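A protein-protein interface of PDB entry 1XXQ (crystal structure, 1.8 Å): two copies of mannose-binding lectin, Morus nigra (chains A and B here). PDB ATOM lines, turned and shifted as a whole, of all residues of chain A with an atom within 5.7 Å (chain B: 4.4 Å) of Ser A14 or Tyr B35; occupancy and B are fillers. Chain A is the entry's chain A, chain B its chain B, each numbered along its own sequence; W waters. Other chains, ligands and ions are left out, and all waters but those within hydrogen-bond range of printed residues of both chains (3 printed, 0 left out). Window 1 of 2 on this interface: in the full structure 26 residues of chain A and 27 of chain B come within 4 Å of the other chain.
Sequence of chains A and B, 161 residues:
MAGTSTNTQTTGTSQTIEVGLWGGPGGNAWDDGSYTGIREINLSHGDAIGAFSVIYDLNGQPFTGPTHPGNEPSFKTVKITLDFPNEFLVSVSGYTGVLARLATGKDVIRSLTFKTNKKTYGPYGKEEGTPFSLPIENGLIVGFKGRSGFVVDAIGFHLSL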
ATOM      1  N   GLY A  12      31.074  16.828  16.617  1.00  0.00           N
ATOM      2  CA  GLY A  12      29.959  16.049  17.130  1.00  0.00           C
ATOM      3  C   GLY A  12      29.370  16.518  18.449  1.00  0.00           C
ATOM      4  O   GLY A  12      28.424  15.916  18.953  1.00  0.00           O
ATOM      5  N   THR A  13      29.910  17.594  19.011  1.00  0.00           N
ATOM      6  CA  THR A  13      29.414  18.112  20.283  1.00  0.00           C
ATOM      7  C   THR A  13      28.540  19.343  20.067  1.00  0.00           C
ATOM      8  O   THR A  13      28.968  20.308  19.432  1.00  0.00           O
ATOM      9  CB  THR A  13      30.587  18.489  21.214  1.00  0.00           C
ATOM     10  OG1 THR A  13      31.421  17.341  21.417  1.00  0.00           O
ATOM     11  CG2 THR A  13      30.074  18.969  22.559  1.00  0.00           C
ATOM     12  N   SER A  14      27.317  19.304  20.590  1.00  0.00           N
ATOM     13  CA  SER A  14      26.398  20.430  20.452  1.00  0.00           C
ATOM     14  C   SER A  14      26.861  21.574  21.346  1.00  0.00           C
ATOM     15  O   SER A  14      27.764  21.404  22.172  1.00  0.00           O
ATOM     16  CB  SER A  14      24.974  20.010  20.837  1.00  0.00           C
ATOM     17  OG  SER A  14      24.893  19.645  22.203  1.00  0.00           O
ATOM     18  N   GLN A  15      26.244  22.741  21.197  1.00  0.00           N
ATOM     19  CA  GLN A  15      26.648  23.880  22.008  1.00  0.00           C
ATOM     20  C   GLN A  15      25.487  24.743  22.480  1.00  0.00           C
ATOM     21  O   GLN A  15      24.345  24.575  22.046  1.00  0.00           O
ATOM     22  CB  GLN A  15      27.632  24.739  21.212  1.00  0.00           C
ATOM     23  CG  GLN A  15      27.010  25.432  20.019  1.00  0.00           C
ATOM     24  CD  GLN A  15      28.043  25.978  19.048  1.00  0.00           C
ATOM     25  OE1 GLN A  15      28.994  26.656  19.448  1.00  0.00           O
ATOM     26  NE2 GLN A  15      27.854  25.691  17.760  1.00  0.00           N
ATOM     27  N   THR A  16      25.795  25.662  23.390  1.00  0.00           N
ATOM     28  CA  THR A  16      24.811  26.601  23.915  1.00  0.00           C
ATOM     29  C   THR A  16      25.482  27.956  24.041  1.00  0.00           C
ATOM     30  O   THR A  16      26.712  28.061  24.032  1.00  0.00           O
ATOM     31  CB  THR A  16      24.315  26.225  25.327  1.00  0.00           C
ATOM     32  OG1 THR A  16      25.433  26.172  26.222  1.00  0.00           O
ATOM     33  CG2 THR A  16      23.599  24.889  25.316  1.00  0.00           C
ATOM     34  N   LEU A  58      17.775  16.841  33.945  1.00  0.00           N
ATOM     35  CA  LEU A  58      18.240  16.272  32.694  1.00  0.00           C
ATOM     36  C   LEU A  58      17.092  15.449  32.148  1.00  0.00           C
ATOM     37  O   LEU A  58      16.925  14.282  32.508  1.00  0.00           O
ATOM     38  CB  LEU A  58      19.466  15.381  32.898  1.00  0.00           C
ATOM     39  CG  LEU A  58      20.011  14.806  31.586  1.00  0.00           C
ATOM     40  CD1 LEU A  58      20.459  15.949  30.668  1.00  0.00           C
ATOM     41  CD2 LEU A  58      21.167  13.872  31.870  1.00  0.00           C
ATOM     42  N   ASN A  59      16.283  16.080  31.304  1.00  0.00           N
ATOM     43  CA  ASN A  59      15.148  15.413  30.689  1.00  0.00           C
ATOM     44  C   ASN A  59      14.174  14.797  31.697  1.00  0.00           C
ATOM     45  O   ASN A  59      13.718  13.665  31.522  1.00  0.00           O
ATOM     46  CB  ASN A  59      15.663  14.350  29.722  1.00  0.00           C
ATOM     47  CG  ASN A  59      16.614  14.927  28.689  1.00  0.00           C
ATOM     48  OD1 ASN A  59      17.746  14.458  28.526  1.00  0.00           O
ATOM     49  ND2 ASN A  59      16.159  15.954  27.984  1.00  0.00           N
ATOM     50  N   ASP B  32      13.683  10.308  24.624  1.00  0.00           N
ATOM     51  CA  ASP B  32      14.901  10.303  25.429  1.00  0.00           C
ATOM     52  C   ASP B  32      15.279  11.693  25.906  1.00  0.00           C
ATOM     53  O   ASP B  32      16.033  11.841  26.862  1.00  0.00           O
ATOM     54  CB  ASP B  32      16.087   9.754  24.636  1.00  0.00           C
ATOM     55  CG  ASP B  32      15.978   8.273  24.356  1.00  0.00           C
ATOM     56  OD1 ASP B  32      15.083   7.614  24.925  1.00  0.00           O
ATOM     57  OD2 ASP B  32      16.804   7.774  23.568  1.00  0.00           O
ATOM     58  N   GLY B  33      14.762  12.712  25.230  1.00  0.00           N
ATOM     59  CA  GLY B  33      15.107  14.069  25.602  1.00  0.00           C
ATOM     60  C   GLY B  33      16.339  14.482  24.817  1.00  0.00           C
ATOM     61  O   GLY B  33      16.671  13.844  23.813  1.00  0.00           O
ATOM     62  N   SER B  34      17.032  15.522  25.278  1.00  0.00           N
ATOM     63  CA  SER B  34      18.213  16.016  24.577  1.00  0.00           C
ATOM     64  C   SER B  34      19.498  15.957  25.393  1.00  0.00           C
ATOM     65  O   SER B  34      19.479  16.051  26.622  1.00  0.00           O
ATOM     66  CB  SER B  34      17.964  17.451  24.097  1.00  0.00           C
ATOM     67  OG  SER B  34      17.503  18.269  25.160  1.00  0.00           O
ATOM     68  N   TYR B  35      20.614  15.814  24.684  1.00  0.00           N
ATOM     69  CA  TYR B  35      21.932  15.711  25.297  1.00  0.00           C
ATOM     70  C   TYR B  35      22.921  16.551  24.486  1.00  0.00           C
ATOM     71  O   TYR B  35      22.516  17.490  23.798  1.00  0.00           O
ATOM     72  CB  TYR B  35      22.359  14.236  25.322  1.00  0.00           C
ATOM     73  CG  TYR B  35      21.329  13.339  25.985  1.00  0.00           C
ATOM     74  CD1 TYR B  35      20.183  12.933  25.299  1.00  0.00           C
ATOM     75  CD2 TYR B  35      21.466  12.954  27.318  1.00  0.00           C
ATOM     76  CE1 TYR B  35      19.193  12.167  25.926  1.00  0.00           C
ATOM     77  CE2 TYR B  35      20.482  12.188  27.957  1.00  0.00           C
ATOM     78  CZ  TYR B  35      19.351  11.802  27.253  1.00  0.00           C
ATOM     79  OH  TYR B  35      18.368  11.060  27.872  1.00  0.00           O
ATOM     80  N   THR B  36      24.208  16.227  24.556  1.00  0.00           N
ATOM     81  CA  THR B  36      25.188  17.000  23.795  1.00  0.00           C
ATOM     82  C   THR B  36      25.760  16.264  22.585  1.00  0.00           C
ATOM     83  O   THR B  36      26.577  16.815  21.847  1.00  0.00           O
ATOM     84  CB  THR B  36      26.351  17.483  24.700  1.00  0.00           C
ATOM     85  OG1 THR B  36      26.988  16.363  25.321  1.00  0.00           O
ATOM     86  CG2 THR B  36      25.819  18.412  25.778  1.00  0.00           C
ATOM     87  N   GLY B  37      25.324  15.027  22.370  1.00  0.00           N
ATOM     88  CA  GLY B  37      25.823  14.268  21.236  1.00  0.00           C
ATOM     89  C   GLY B  37      25.456  12.797  21.285  1.00  0.00           C
ATOM     90  O   GLY B  37      24.770  12.359  22.205  1.00  0.00           O
ATOM     91  N   TYR B  56      24.240   8.390  24.838  1.00  0.00           N
ATOM     92  CA  TYR B  56      24.513   9.757  24.430  1.00  0.00           C
ATOM     93  C   TYR B  56      25.764  10.302  25.071  1.00  0.00           C
ATOM     94  O   TYR B  56      26.379   9.665  25.931  1.00  0.00           O
ATOM     95  CB  TYR B  56      23.359  10.674  24.845  1.00  0.00           C
ATOM     96  CG  TYR B  56      22.032  10.325  24.231  1.00  0.00           C
ATOM     97  CD1 TYR B  56      21.126   9.492  24.888  1.00  0.00           C
ATOM     98  CD2 TYR B  56      21.685  10.827  22.980  1.00  0.00           C
ATOM     99  CE1 TYR B  56      19.895   9.169  24.303  1.00  0.00           C
ATOM    100  CE2 TYR B  56      20.475  10.514  22.393  1.00  0.00           C
ATOM    101  CZ  TYR B  56      19.585   9.688  23.051  1.00  0.00           C
ATOM    102  OH  TYR B  56      18.393   9.387  22.437  1.00  0.00           O
ATOM    103  N   ASP B  57      26.149  11.489  24.626  1.00  0.00           N
ATOM    104  CA  ASP B  57      27.270  12.161  25.238  1.00  0.00           C
ATOM    105  C   ASP B  57      26.595  13.237  26.057  1.00  0.00           C
ATOM    106  O   ASP B  57      25.627  13.849  25.605  1.00  0.00           O
ATOM    107  CB  ASP B  57      28.179  12.852  24.230  1.00  0.00           C
ATOM    108  CG  ASP B  57      29.292  13.623  24.919  1.00  0.00           C
ATOM    109  OD1 ASP B  57      30.154  12.967  25.537  1.00  0.00           O
ATOM    110  OD2 ASP B  57      29.292  14.872  24.868  1.00  0.00           O
ATOM    111  N   PHE B  63      26.426   8.877  28.571  1.00  0.00           N
ATOM    112  CA  PHE B  63      25.211   8.837  29.367  1.00  0.00           C
ATOM    113  C   PHE B  63      24.249   7.897  28.656  1.00  0.00           C
ATOM    114  O   PHE B  63      23.792   8.174  27.545  1.00  0.00           O
ATOM    115  CB  PHE B  63      24.559  10.214  29.497  1.00  0.00           C
ATOM    116  CG  PHE B  63      23.367  10.221  30.409  1.00  0.00           C
ATOM    117  CD1 PHE B  63      23.516  10.459  31.771  1.00  0.00           C
ATOM    118  CD2 PHE B  63      22.099   9.934  29.918  1.00  0.00           C
ATOM    119  CE1 PHE B  63      22.419  10.410  32.629  1.00  0.00           C
ATOM    120  CE2 PHE B  63      20.996   9.882  30.768  1.00  0.00           C
ATOM    121  CZ  PHE B  63      21.159  10.120  32.127  1.00  0.00           C
ATOM    122  N   PRO B  66      17.365   5.840  28.137  1.00  0.00           N
ATOM    123  CA  PRO B  66      16.456   4.737  28.446  1.00  0.00           C
ATOM    124  C   PRO B  66      16.412   3.784  27.257  1.00  0.00           C
ATOM    125  O   PRO B  66      16.609   4.188  26.107  1.00  0.00           O
ATOM    126  CB  PRO B  66      15.120   5.439  28.707  1.00  0.00           C
ATOM    127  CG  PRO B  66      15.247   6.735  27.980  1.00  0.00           C
ATOM    128  CD  PRO B  66      16.672   7.138  28.212  1.00  0.00           C
ATOM    129  N   LEU B 140      23.175  19.152  14.793  1.00  0.00           N
ATOM    130  CA  LEU B 140      23.384  17.770  15.215  1.00  0.00           C
ATOM    131  C   LEU B 140      22.142  17.140  15.825  1.00  0.00           C
ATOM    132  O   LEU B 140      21.297  17.834  16.389  1.00  0.00           O
ATOM    133  CB  LEU B 140      24.475  17.718  16.289  1.00  0.00           C
ATOM    134  CG  LEU B 140      25.923  18.092  15.978  1.00  0.00           C
ATOM    135  CD1 LEU B 140      26.684  18.310  17.281  1.00  0.00           C
ATOM    136  CD2 LEU B 140      26.564  16.982  15.152  1.00  0.00           C
ATOM    137  N   VAL B 142      20.709  15.466  18.768  1.00  0.00           N
ATOM    138  CA  VAL B 142      21.147  15.390  20.160  1.00  0.00           C
ATOM    139  C   VAL B 142      20.190  14.569  21.016  1.00  0.00           C
ATOM    140  O   VAL B 142      20.281  14.564  22.244  1.00  0.00           O
ATOM    141  CB  VAL B 142      21.290  16.801  20.781  1.00  0.00           C
ATOM    142  CG1 VAL B 142      22.428  17.551  20.101  1.00  0.00           C
ATOM    143  CG2 VAL B 142      19.986  17.577  20.630  1.00  0.00           C
ATOM    144  N   SER B 160      20.062  20.334  17.430  1.00  0.00           N
ATOM    145  CA  SER B 160      20.683  21.487  18.073  1.00  0.00           C
ATOM    146  C   SER B 160      21.958  21.900  17.361  1.00  0.00           C
ATOM    147  O   SER B 160      22.597  21.092  16.690  1.00  0.00           O
ATOM    148  CB  SER B 160      21.030  21.168  19.530  1.00  0.00           C
ATOM    149  OG  SER B 160      21.820  22.207  20.095  1.00  0.00           O
ATOM    150  N   LEU B 161      22.317  23.170  17.505  1.00  0.00           N
ATOM    151  CA  LEU B 161      23.553  23.679  16.928  1.00  0.00           C
ATOM    152  C   LEU B 161      24.654  23.303  17.919  1.00  0.00           C
ATOM    153  O   LEU B 161      25.850  23.464  17.590  1.00  0.00           O
ATOM    154  CB  LEU B 161      23.486  25.201  16.772  1.00  0.00           C
ATOM    155  CG  LEU B 161      22.569  25.712  15.659  1.00  0.00           C
ATOM    156  CD1 LEU B 161      22.461  27.231  15.731  1.00  0.00           C
ATOM    157  CD2 LEU B 161      23.115  25.268  14.307  1.00  0.00           C
ATOM    158  OXT LEU B 161      24.291  22.848  19.025  1.00  0.00           O
HETATM  159  O   HOH W   1      31.349  16.410  24.268  1.00  0.00           O
HETATM  160  O   HOH W   2      28.055  22.042  17.397  1.00  0.00           O
HETATM  161  O   HOH W   3      18.000  11.792  30.401  1.00  0.00           O
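The backbone NH (N) of Ser B34 sits close to the side-chain amide nitrogen (ND2) of Asn A59.
N of Gln A15 lies within hydrogen-bond range of OXT of Leu B161, 2.9 Å away.
The backbone NH of Ser A14 sits at hydrogen-bond distance from the backbone carbonyl oxygen of Thr B36 (2.9 Å).
Of the 7 printed residues of chain A, 6 touch a printed residue of chain B.
Among the printed residues, no Asp or Glu carboxylate lies within 4 Å of a Lys or Arg side-chain nitrogen of the other chain.
Of chain B, only Tyr B35 (3.6 Å), Thr B36 (2.9 Å), Leu B140 (3.5 Å), Val B142 (3.6 Å), Ser B160 (3.9 Å) and Leu B161 (3.4 Å) come within 4 Å of Ser A14.
Of the printed residues of chain A, Ser B34 touches Asn A59 (2.9 Å).
Tyr B35 touches two residues of chain A.
Pro B66 touches none of the printed residues of chain A.
Printed residues of chain A within 4 Å of Leu B140: Gly A12, Thr A13 and Ser A14.
Printed residues of chain A within 4 Å of Val B142: Ser A14.
Of the printed residues of chain A, Ser B160 touches Ser A14 (3.9 Å) and Gln A15 (3.97 Å).
The nearest printed residue of chain A that does not touch Ser B34 is Leu A58 (4.2 Å).
Water W2 bridges O of Leu B161 (2.6 Å) and O of Thr A13 (2.8 Å).
Water W1 lies within hydrogen-bond range of the side-chain carboxylate (OD2) of Asp B57 (2.6 Å) and the side-chain hydroxyl (OG1) of Thr A13 (3.0 Å).
Water W3 lies within hydrogen-bond range of the side-chain hydroxyl of Tyr B35, the side-chain amide oxygen of Asn A59 and the backbone carbonyl oxygen of Leu A58.
No position is printed for both chains.
O of Gly A12 touches O of Thr B36, 3.5 Å away.
Gly A12 touches Leu B140.
Thr B36 touches Thr A13 (O to CA, 3.5 Å).
Tyr B35 touches Ser A14 (O to OG, 3.6 Å).
N of Ser A14 touches CD1 of Leu B140, 3.5 Å away.
CB of Ser A14 touches CG1 of Val B142, 3.6 Å away.
CB of Ser A14 touches OXT of Leu B161 (3.4 Å).
Ser B160 touches Gln A15 (OG to O, 3.97 Å).
Asp B32 touches Asn A59 (O to OD1, 3.5 Å).
ND2 of Asn A59 touches CA of Gly B33, 3.2 Å away.
The backbone carbonyl oxygen (O) of Gly B37 sits at hydrogen-bond distance from the backbone NH (N) of Asp B57 (2.9 Å).
N of Leu B140 is in hydrogen-bond range of O of Ser B160, 2.8 Å away.
The backbone NH of Tyr B35 lies within hydrogen-bond range of the backbone carbonyl oxygen of Val B142 (2.8 Å).
OD2 of Asp B32 lies within hydrogen-bond range of OH of Tyr B56.
The side-chain carboxylate of Asp B57 lies within hydrogen-bond range of the side-chain hydroxyl of Thr B36 (2.8 Å).
O of Asp B32 sits at hydrogen-bond distance from OH of Tyr B35.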
